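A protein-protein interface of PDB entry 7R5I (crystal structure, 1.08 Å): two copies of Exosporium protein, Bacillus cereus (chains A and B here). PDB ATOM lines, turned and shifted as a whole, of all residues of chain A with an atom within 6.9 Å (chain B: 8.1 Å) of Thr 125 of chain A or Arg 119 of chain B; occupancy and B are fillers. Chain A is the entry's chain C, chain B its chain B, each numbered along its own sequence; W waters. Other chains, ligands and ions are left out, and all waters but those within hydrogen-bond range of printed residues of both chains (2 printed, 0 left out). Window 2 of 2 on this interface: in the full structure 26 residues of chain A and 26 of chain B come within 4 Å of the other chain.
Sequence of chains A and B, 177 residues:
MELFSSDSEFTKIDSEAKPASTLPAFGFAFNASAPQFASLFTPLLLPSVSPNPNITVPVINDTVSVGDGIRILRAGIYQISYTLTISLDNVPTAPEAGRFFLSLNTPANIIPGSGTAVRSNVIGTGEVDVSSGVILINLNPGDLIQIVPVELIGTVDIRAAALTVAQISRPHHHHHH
NH1 of Arg 99 of chain B is in salt-bridge range of OE1 of Glu 127 of chain A, at 3.1 Å. NE of Arg 99 of chain B lies within salt-bridge range of OD2 of Asp 129 of chain A (2.8 Å). The side-chain carboxylate (OD2) of Asp 129 of chain A lies close to the backbone NH (N) of Thr 116 of chain B (3.3 Å). O of Glu 127 of chain A lies within hydrogen-bond range of NE of Arg 119 of chain B (2.9 Å).
The backbone NH of Val 150 of chain B sits at hydrogen-bond distance from the backbone carbonyl oxygen of Arg 99 of chain B, at 2.8 Å. The backbone NH of Arg 99 of chain B is in hydrogen-bond range of the backbone carbonyl oxygen of Glu 151 of chain B, at 2.9 Å. The backbone carbonyl oxygen (O) of Phe 100 of chain B is in hydrogen-bond range of the backbone NH (N) of Thr 116 of chain B, at 2.9 Å. NH2 of Arg 119 of chain B lies within salt-bridge range of OE1 of Glu 151 of chain B, 3.0 Å away.
Among the printed residues, pairs that only touch across the chains: Gly 126 of chain A with Arg 119 of chain B (3.5 Å), Thr 125 of chain A with Arg 119 of chain B (3.6 Å), Asp 129 of chain A with Ala 117 of chain B (3.6 Å), Glu 127 of chain A with Ala 117 of chain B (3.9 Å) and Val 128 of chain A with Arg 119 of chain B (3.997 Å).
Thr 125 of chain A touches just one residue of chain B: Arg 119 (3.6 Å). Of chain B, only Arg 119 comes within 4 Å of Gly 126 of chain A. Printed residues of chain B within 4 Å of Glu 127 of chain A: Arg 99 (3.1 Å), Ala 117 (3.9 Å) and Arg 119 (2.9 Å). Printed residues of chain B within 4 Å of Asp 129 of chain A: Arg 99, Thr 116 and Ala 117. Ile 86 of chain B touches none of the printed residues of chain A. Ala 97 of chain B touches none of the printed residues of chain A. Of the printed residues of chain A, Thr 116 of chain B touches Asp 129. Of the printed residues of chain A, Arg 119 of chain B touches Thr 125 (3.6 Å), Gly 126 (3.5 Å), Glu 127 (2.9 Å) and Val 128 (3.997 Å). The nearest printed residue of chain B that does not touch Thr 125 of chain A is Ala 97 of chain B (7.1 Å). The nearest printed residue of chain A that does not touch Arg 119 of chain B is Asp 129 of chain A (6.9 Å).
Of the 18 printed residues of chain B, 4 touch a printed residue of chain A. Hydrophobic or aromatic side chains of chain B within 4 Å of the printed part of chain A: Ala 117. Printed residues of chain A that touch a printed residue of chain B: Thr 125, Gly 126, Glu 127, Val 128 and Asp 129. Among the printed residues, 9 pairs touch across the chains. Among the printed residues, Asp or Glu carboxylates within 4 Å of a Lys or Arg side-chain nitrogen of the other chain: Glu 127 of chain A with Arg 99 of chain B (3.1 Å) and Asp 129 of chain A with Arg 99 of chain B (2.8 Å).
2 positions are printed for both chains. Of the 9 pairs that touch across the chains among the printed residues, none has its exchanged pair printed and touching as well.
Water W2 lies within hydrogen-bond range of the backbone carbonyl oxygen of Ala 117 of chain B and the backbone carbonyl oxygen of Asp 129 of chain A. Water W1 lies within hydrogen-bond range of N of Ala 117 of chain B (2.9 Å) and O of Asp 129 of chain A (3.2 Å).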
ATOM      1  N   SER A  87       7.228  31.806  26.062  1.00  0.00           N
ATOM      2  CA  SER A  87       6.622  30.914  25.043  1.00  0.00           C
ATOM      3  C   SER A  87       5.576  31.724  24.282  1.00  0.00           C
ATOM      4  O   SER A  87       4.628  32.209  24.925  1.00  0.00           O
ATOM      5  CB  SER A  87       6.025  29.688  25.674  1.00  0.00           C
ATOM      6  OG  SER A  87       5.607  28.766  24.679  1.00  0.00           O
ATOM      7  N   LEU A  88       5.759  31.885  22.971  1.00  0.00           N
ATOM      8  CA  LEU A  88       4.830  32.750  22.200  1.00  0.00           C
ATOM      9  C   LEU A  88       4.093  31.943  21.133  1.00  0.00           C
ATOM     10  O   LEU A  88       4.699  31.012  20.572  1.00  0.00           O
ATOM     11  CB  LEU A  88       5.632  33.870  21.530  1.00  0.00           C
ATOM     12  CG  LEU A  88       6.284  34.880  22.472  1.00  0.00           C
ATOM     13  CD1 LEU A  88       7.061  35.922  21.684  1.00  0.00           C
ATOM     14  CD2 LEU A  88       5.240  35.550  23.352  1.00  0.00           C
ATOM     15  N   ASP A  89       2.827  32.276  20.891  1.00  0.00           N
ATOM     16  CA  ASP A  89       2.074  31.657  19.770  1.00  0.00           C
ATOM     17  C   ASP A  89       2.418  32.518  18.558  1.00  0.00           C
ATOM     18  O   ASP A  89       2.482  33.751  18.740  1.00  0.00           O
ATOM     19  CB  ASP A  89       0.582  31.611  20.098  1.00  0.00           C
ATOM     20  CG  ASP A  89       0.333  31.113  21.508  1.00  0.00           C
ATOM     21  OD1 ASP A  89       0.901  30.050  21.849  1.00  0.00           O
ATOM     22  OD2 ASP A  89      -0.353  31.830  22.271  1.00  0.00           O
ATOM     23  N   ASN A  90       2.739  31.949  17.402  1.00  0.00           N
ATOM     24  CA  ASN A  90       2.856  32.842  16.227  1.00  0.00           C
ATOM     25  C   ASN A  90       1.618  32.644  15.355  1.00  0.00           C
ATOM     26  O   ASN A  90       1.665  31.845  14.412  1.00  0.00           O
ATOM     27  CB  ASN A  90       4.162  32.755  15.444  1.00  0.00           C
ATOM     28  CG  ASN A  90       4.301  33.976  14.550  1.00  0.00           C
ATOM     29  OD1 ASN A  90       3.796  35.061  14.878  1.00  0.00           O
ATOM     30  ND2 ASN A  90       4.942  33.804  13.405  1.00  0.00           N
ATOM     31  N   SER A 120       6.967  37.366  18.210  1.00  0.00           N
ATOM     32  CA  SER A 120       6.584  36.128  17.481  1.00  0.00           C
ATOM     33  C   SER A 120       6.863  36.267  15.972  1.00  0.00           C
ATOM     34  O   SER A 120       7.183  35.208  15.416  1.00  0.00           O
ATOM     35  CB  SER A 120       5.169  35.820  17.777  1.00  0.00           C
ATOM     36  OG  SER A 120       4.350  36.817  17.205  1.00  0.00           O
ATOM     37  N   THR A 125       7.541  29.870  17.575  1.00  0.00           N
ATOM     38  CA  THR A 125       6.884  28.883  18.469  1.00  0.00           C
ATOM     39  C   THR A 125       7.967  28.037  19.162  1.00  0.00           C
ATOM     40  O   THR A 125       8.951  27.689  18.490  1.00  0.00           O
ATOM     41  CB  THR A 125       5.860  28.028  17.702  1.00  0.00           C
ATOM     42  OG1 THR A 125       5.215  27.172  18.649  1.00  0.00           O
ATOM     43  CG2 THR A 125       6.456  27.185  16.594  1.00  0.00           C
ATOM     44  N   GLY A 126       7.801  27.787  20.465  1.00  0.00           N
ATOM     45  CA  GLY A 126       8.815  27.054  21.250  1.00  0.00           C
ATOM     46  C   GLY A 126       9.402  27.959  22.325  1.00  0.00           C
ATOM     47  O   GLY A 126       9.517  29.166  22.070  1.00  0.00           O
ATOM     48  N   GLU A 127       9.742  27.401  23.490  1.00  0.00           N
ATOM     49  CA  GLU A 127      10.296  28.218  24.603  1.00  0.00           C
ATOM     50  C   GLU A 127      11.557  28.940  24.112  1.00  0.00           C
ATOM     51  O   GLU A 127      12.450  28.265  23.565  1.00  0.00           O
ATOM     52  CB  GLU A 127      10.597  27.353  25.829  1.00  0.00           C
ATOM     53  CG  GLU A 127       9.373  27.055  26.676  1.00  0.00           C
ATOM     54  CD  GLU A 127       9.676  26.359  27.991  1.00  0.00           C
ATOM     55  OE1 GLU A 127      10.771  25.776  28.111  1.00  0.00           O
ATOM     56  OE2 GLU A 127       8.818  26.408  28.894  1.00  0.00           O
ATOM     57  N   VAL A 128      11.617  30.261  24.305  1.00  0.00           N
ATOM     58  CA  VAL A 128      12.816  31.053  23.899  1.00  0.00           C
ATOM     59  C   VAL A 128      13.316  31.828  25.117  1.00  0.00           C
ATOM     60  O   VAL A 128      12.479  32.241  25.938  1.00  0.00           O
ATOM     61  CB  VAL A 128      12.504  32.000  22.726  1.00  0.00           C
ATOM     62  CG1 VAL A 128      12.153  31.231  21.461  1.00  0.00           C
ATOM     63  CG2 VAL A 128      11.405  32.990  23.076  1.00  0.00           C
ATOM     64  N   ASP A 129      14.631  32.017  25.222  1.00  0.00           N
ATOM     65  CA  ASP A 129      15.191  32.701  26.364  1.00  0.00           C
ATOM     66  C   ASP A 129      15.737  34.050  25.883  1.00  0.00           C
ATOM     67  O   ASP A 129      16.257  34.144  24.732  1.00  0.00           O
ATOM     68  CB  ASP A 129      16.350  31.874  26.910  1.00  0.00           C
ATOM     69  CG  ASP A 129      15.940  30.539  27.475  1.00  0.00           C
ATOM     70  OD1 ASP A 129      15.371  30.524  28.621  1.00  0.00           O
ATOM     71  OD2 ASP A 129      16.164  29.563  26.773  1.00  0.00           O
ATOM     72  N   ILE B  86      26.127  29.985  16.896  1.00  0.00           N
ATOM     73  CA  ILE B  86      25.602  28.907  16.058  1.00  0.00           C
ATOM     74  C   ILE B  86      25.629  29.332  14.597  1.00  0.00           C
ATOM     75  O   ILE B  86      25.209  30.489  14.290  1.00  0.00           O
ATOM     76  CB  ILE B  86      24.196  28.510  16.532  1.00  0.00           C
ATOM     77  CG1 ILE B  86      24.203  27.816  17.901  1.00  0.00           C
ATOM     78  CG2 ILE B  86      23.550  27.647  15.493  1.00  0.00           C
ATOM     79  CD1 ILE B  86      24.474  28.695  19.043  1.00  0.00           C
ATOM     80  N   LEU B  88      23.661  28.903  11.627  1.00  0.00           N
ATOM     81  CA  LEU B  88      22.282  28.463  11.308  1.00  0.00           C
ATOM     82  C   LEU B  88      22.171  28.319   9.798  1.00  0.00           C
ATOM     83  O   LEU B  88      22.674  29.194   9.055  1.00  0.00           O
ATOM     84  CB  LEU B  88      21.269  29.490  11.819  1.00  0.00           C
ATOM     85  CG  LEU B  88      20.684  29.239  13.203  1.00  0.00           C
ATOM     86  CD1 LEU B  88      19.534  30.204  13.433  1.00  0.00           C
ATOM     87  CD2 LEU B  88      20.213  27.798  13.413  1.00  0.00           C
ATOM     88  N   PRO B  95      14.559  22.916   9.126  1.00  0.00           N
ATOM     89  CA  PRO B  95      14.538  23.752  10.345  1.00  0.00           C
ATOM     90  C   PRO B  95      15.565  23.275  11.380  1.00  0.00           C
ATOM     91  O   PRO B  95      15.837  22.097  11.506  1.00  0.00           O
ATOM     92  CB  PRO B  95      13.136  23.669  10.975  1.00  0.00           C
ATOM     93  CG  PRO B  95      12.308  23.072   9.875  1.00  0.00           C
ATOM     94  CD  PRO B  95      13.278  22.210   9.080  1.00  0.00           C
ATOM     95  N   GLU B  96      16.133  24.230  12.116  1.00  0.00           N
ATOM     96  CA  GLU B  96      17.231  23.981  13.070  1.00  0.00           C
ATOM     97  C   GLU B  96      16.869  24.751  14.337  1.00  0.00           C
ATOM     98  O   GLU B  96      16.519  25.916  14.262  1.00  0.00           O
ATOM     99  CB  GLU B  96      18.595  24.404  12.487  1.00  0.00           C
ATOM    100  CG  GLU B  96      19.031  23.586  11.272  1.00  0.00           C
ATOM    101  CD  GLU B  96      20.381  23.928  10.652  1.00  0.00           C
ATOM    102  OE1 GLU B  96      20.865  23.109   9.790  1.00  0.00           O
ATOM    103  OE2 GLU B  96      20.947  25.010  10.995  1.00  0.00           O
ATOM    104  N   ALA B  97      16.941  24.098  15.490  1.00  0.00           N
ATOM    105  CA  ALA B  97      16.703  24.753  16.787  1.00  0.00           C
ATOM    106  C   ALA B  97      17.517  24.027  17.869  1.00  0.00           C
ATOM    107  O   ALA B  97      17.714  22.760  17.775  1.00  0.00           O
ATOM    108  CB  ALA B  97      15.236  24.714  17.122  1.00  0.00           C
ATOM    109  N   GLY B  98      17.885  24.737  18.909  1.00  0.00           N
ATOM    110  CA  GLY B  98      18.540  24.109  20.060  1.00  0.00           C
ATOM    111  C   GLY B  98      18.168  24.837  21.324  1.00  0.00           C
ATOM    112  O   GLY B  98      17.994  26.070  21.339  1.00  0.00           O
ATOM    113  N   ARG B  99      18.189  24.102  22.428  1.00  0.00           N
ATOM    114  CA  ARG B  99      18.093  24.669  23.782  1.00  0.00           C
ATOM    115  C   ARG B  99      19.277  24.127  24.560  1.00  0.00           C
ATOM    116  O   ARG B  99      19.580  22.910  24.424  1.00  0.00           O
ATOM    117  CB  ARG B  99      16.789  24.194  24.441  1.00  0.00           C
ATOM    118  CG  ARG B  99      16.453  24.930  25.725  1.00  0.00           C
ATOM    119  CD  ARG B  99      15.461  26.070  25.483  1.00  0.00           C
ATOM    120  NE  ARG B  99      15.337  26.919  26.650  1.00  0.00           N
ATOM    121  CZ  ARG B  99      14.562  26.670  27.701  1.00  0.00           C
ATOM    122  NH1 ARG B  99      13.833  25.571  27.753  1.00  0.00           N
ATOM    123  NH2 ARG B  99      14.605  27.510  28.731  1.00  0.00           N
ATOM    124  N   PHE B 100      19.847  24.956  25.377  1.00  0.00           N
ATOM    125  CA  PHE B 100      21.047  24.629  26.147  1.00  0.00           C
ATOM    126  C   PHE B 100      20.885  25.100  27.575  1.00  0.00           C
ATOM    127  O   PHE B 100      20.140  26.044  27.844  1.00  0.00           O
ATOM    128  CB  PHE B 100      22.294  25.312  25.552  1.00  0.00           C
ATOM    129  CG  PHE B 100      22.414  25.037  24.076  1.00  0.00           C
ATOM    130  CD1 PHE B 100      21.751  25.841  23.162  1.00  0.00           C
ATOM    131  CD2 PHE B 100      23.203  24.017  23.583  1.00  0.00           C
ATOM    132  CE1 PHE B 100      21.848  25.602  21.793  1.00  0.00           C
ATOM    133  CE2 PHE B 100      23.304  23.783  22.222  1.00  0.00           C
ATOM    134  CZ  PHE B 100      22.644  24.593  21.337  1.00  0.00           C
ATOM    135  N   THR B 116      19.371  28.834  27.403  1.00  0.00           N
ATOM    136  CA  THR B 116      19.444  29.626  26.174  1.00  0.00           C
ATOM    137  C   THR B 116      18.756  28.849  25.083  1.00  0.00           C
ATOM    138  O   THR B 116      18.575  27.596  25.178  1.00  0.00           O
ATOM    139  CB  THR B 116      20.886  29.903  25.726  1.00  0.00           C
ATOM    140  OG1 THR B 116      21.606  28.695  25.553  1.00  0.00           O
ATOM    141  CG2 THR B 116      21.606  30.832  26.666  1.00  0.00           C
ATOM    142  N   ALA B 117      18.415  29.533  23.998  1.00  0.00           N
ATOM    143  CA  ALA B 117      17.735  28.875  22.873  1.00  0.00           C
ATOM    144  C   ALA B 117      18.072  29.587  21.575  1.00  0.00           C
ATOM    145  O   ALA B 117      18.224  30.826  21.550  1.00  0.00           O
ATOM    146  CB  ALA B 117      16.235  28.896  23.074  1.00  0.00           C
ATOM    147  N   VAL B 118      18.113  28.802  20.515  1.00  0.00           N
ATOM    148  CA  VAL B 118      18.173  29.302  19.124  1.00  0.00           C
ATOM    149  C   VAL B 118      17.032  28.646  18.319  1.00  0.00           C
ATOM    150  O   VAL B 118      16.981  27.411  18.311  1.00  0.00           O
ATOM    151  CB  VAL B 118      19.560  29.013  18.518  1.00  0.00           C
ATOM    152  CG1 VAL B 118      19.606  29.359  17.039  1.00  0.00           C
ATOM    153  CG2 VAL B 118      20.666  29.726  19.277  1.00  0.00           C
ATOM    154  N   ARG B 119      16.187  29.442  17.638  1.00  0.00           N
ATOM    155  CA  ARG B 119      15.000  28.911  16.883  1.00  0.00           C
ATOM    156  C   ARG B 119      14.711  29.799  15.667  1.00  0.00           C
ATOM    157  O   ARG B 119      15.711  30.012  14.927  1.00  0.00           O
ATOM    158  CB  ARG B 119      13.730  28.865  17.740  1.00  0.00           C
ATOM    159  CG  ARG B 119      13.778  27.980  18.976  1.00  0.00           C
ATOM    160  CD  ARG B 119      12.364  27.760  19.490  1.00  0.00           C
ATOM    161  NE  ARG B 119      12.442  27.197  20.824  1.00  0.00           N
ATOM    162  CZ  ARG B 119      12.626  25.903  21.114  1.00  0.00           C
ATOM    163  NH1 ARG B 119      12.719  24.987  20.153  1.00  0.00           N
ATOM    164  NH2 ARG B 119      12.744  25.551  22.389  1.00  0.00           N
ATOM    165  N   VAL B 128      24.767  33.329  14.419  1.00  0.00           N
ATOM    166  CA  VAL B 128      24.002  34.037  15.466  1.00  0.00           C
ATOM    167  C   VAL B 128      24.570  33.685  16.834  1.00  0.00           C
ATOM    168  O   VAL B 128      25.049  32.573  17.072  1.00  0.00           O
ATOM    169  CB  VAL B 128      22.511  33.748  15.429  1.00  0.00           C
ATOM    170  CG1 VAL B 128      21.955  34.034  14.062  1.00  0.00           C
ATOM    171  CG2 VAL B 128      22.185  32.331  15.826  1.00  0.00           C
ATOM    172  N   VAL B 130      24.239  33.752  21.120  1.00  0.00           N
ATOM    173  CA  VAL B 130      23.312  33.740  22.268  1.00  0.00           C
ATOM    174  C   VAL B 130      24.148  33.844  23.525  1.00  0.00           C
ATOM    175  O   VAL B 130      25.314  33.419  23.573  1.00  0.00           O
ATOM    176  CB  VAL B 130      22.401  32.513  22.330  1.00  0.00           C
ATOM    177  CG1 VAL B 130      21.484  32.417  21.140  1.00  0.00           C
ATOM    178  CG2 VAL B 130      23.218  31.267  22.466  1.00  0.00           C
ATOM    179  N   VAL B 150      20.035  20.389  25.567  1.00  0.00           N
ATOM    180  CA  VAL B 150      18.911  19.608  26.159  1.00  0.00           C
ATOM    181  C   VAL B 150      17.799  19.332  25.146  1.00  0.00           C
ATOM    182  O   VAL B 150      16.918  18.488  25.446  1.00  0.00           O
ATOM    183  CB  VAL B 150      18.355  20.284  27.418  1.00  0.00           C
ATOM    184  CG1 VAL B 150      19.477  20.529  28.402  1.00  0.00           C
ATOM    185  CG2 VAL B 150      17.591  21.546  27.131  1.00  0.00           C
ATOM    186  N   GLU B 151      17.765  20.006  24.014  1.00  0.00           N
ATOM    187  CA  GLU B 151      16.753  19.882  22.940  1.00  0.00           C
ATOM    188  C   GLU B 151      17.461  20.267  21.638  1.00  0.00           C
ATOM    189  O   GLU B 151      18.097  21.303  21.588  1.00  0.00           O
ATOM    190  CB  GLU B 151      15.522  20.773  23.207  1.00  0.00           C
ATOM    191  CG  GLU B 151      14.408  20.709  22.145  1.00  0.00           C
ATOM    192  CD  GLU B 151      13.434  21.887  22.163  1.00  0.00           C
ATOM    193  OE1 GLU B 151      13.487  22.740  23.107  1.00  0.00           O
ATOM    194  OE2 GLU B 151      12.673  22.023  21.188  1.00  0.00           O
ATOM    195  N   LEU B 152      17.306  19.425  20.624  1.00  0.00           N
ATOM    196  CA  LEU B 152      17.861  19.707  19.280  1.00  0.00           C
ATOM    197  C   LEU B 152      16.866  19.309  18.199  1.00  0.00           C
ATOM    198  O   LEU B 152      16.320  18.216  18.250  1.00  0.00           O
ATOM    199  CB  LEU B 152      19.158  18.928  19.116  1.00  0.00           C
ATOM    200  CG  LEU B 152      20.306  19.378  20.029  1.00  0.00           C
ATOM    201  CD1 LEU B 152      21.437  18.361  19.965  1.00  0.00           C
ATOM    202  CD2 LEU B 152      20.846  20.771  19.678  1.00  0.00           C
ATOM    203  N   ILE B 153      16.657  20.217  17.258  1.00  0.00           N
ATOM    204  CA  ILE B 153      15.855  19.982  16.029  1.00  0.00           C
ATOM    205  C   ILE B 153      16.799  20.184  14.866  1.00  0.00           C
ATOM    206  O   ILE B 153      17.393  21.238  14.795  1.00  0.00           O
ATOM    207  CB  ILE B 153      14.633  20.935  15.996  1.00  0.00           C
ATOM    208  CG1 ILE B 153      13.700  20.664  17.188  1.00  0.00           C
ATOM    209  CG2 ILE B 153      13.884  20.796  14.675  1.00  0.00           C
ATOM    210  CD1 ILE B 153      12.573  21.692  17.368  1.00  0.00           C
HETATM  211  O   HOH W   1      18.894  32.404  24.282  1.00  0.00           O
HETATM  212  O   HOH W   2      16.068  32.287  22.512  1.00  0.00           O
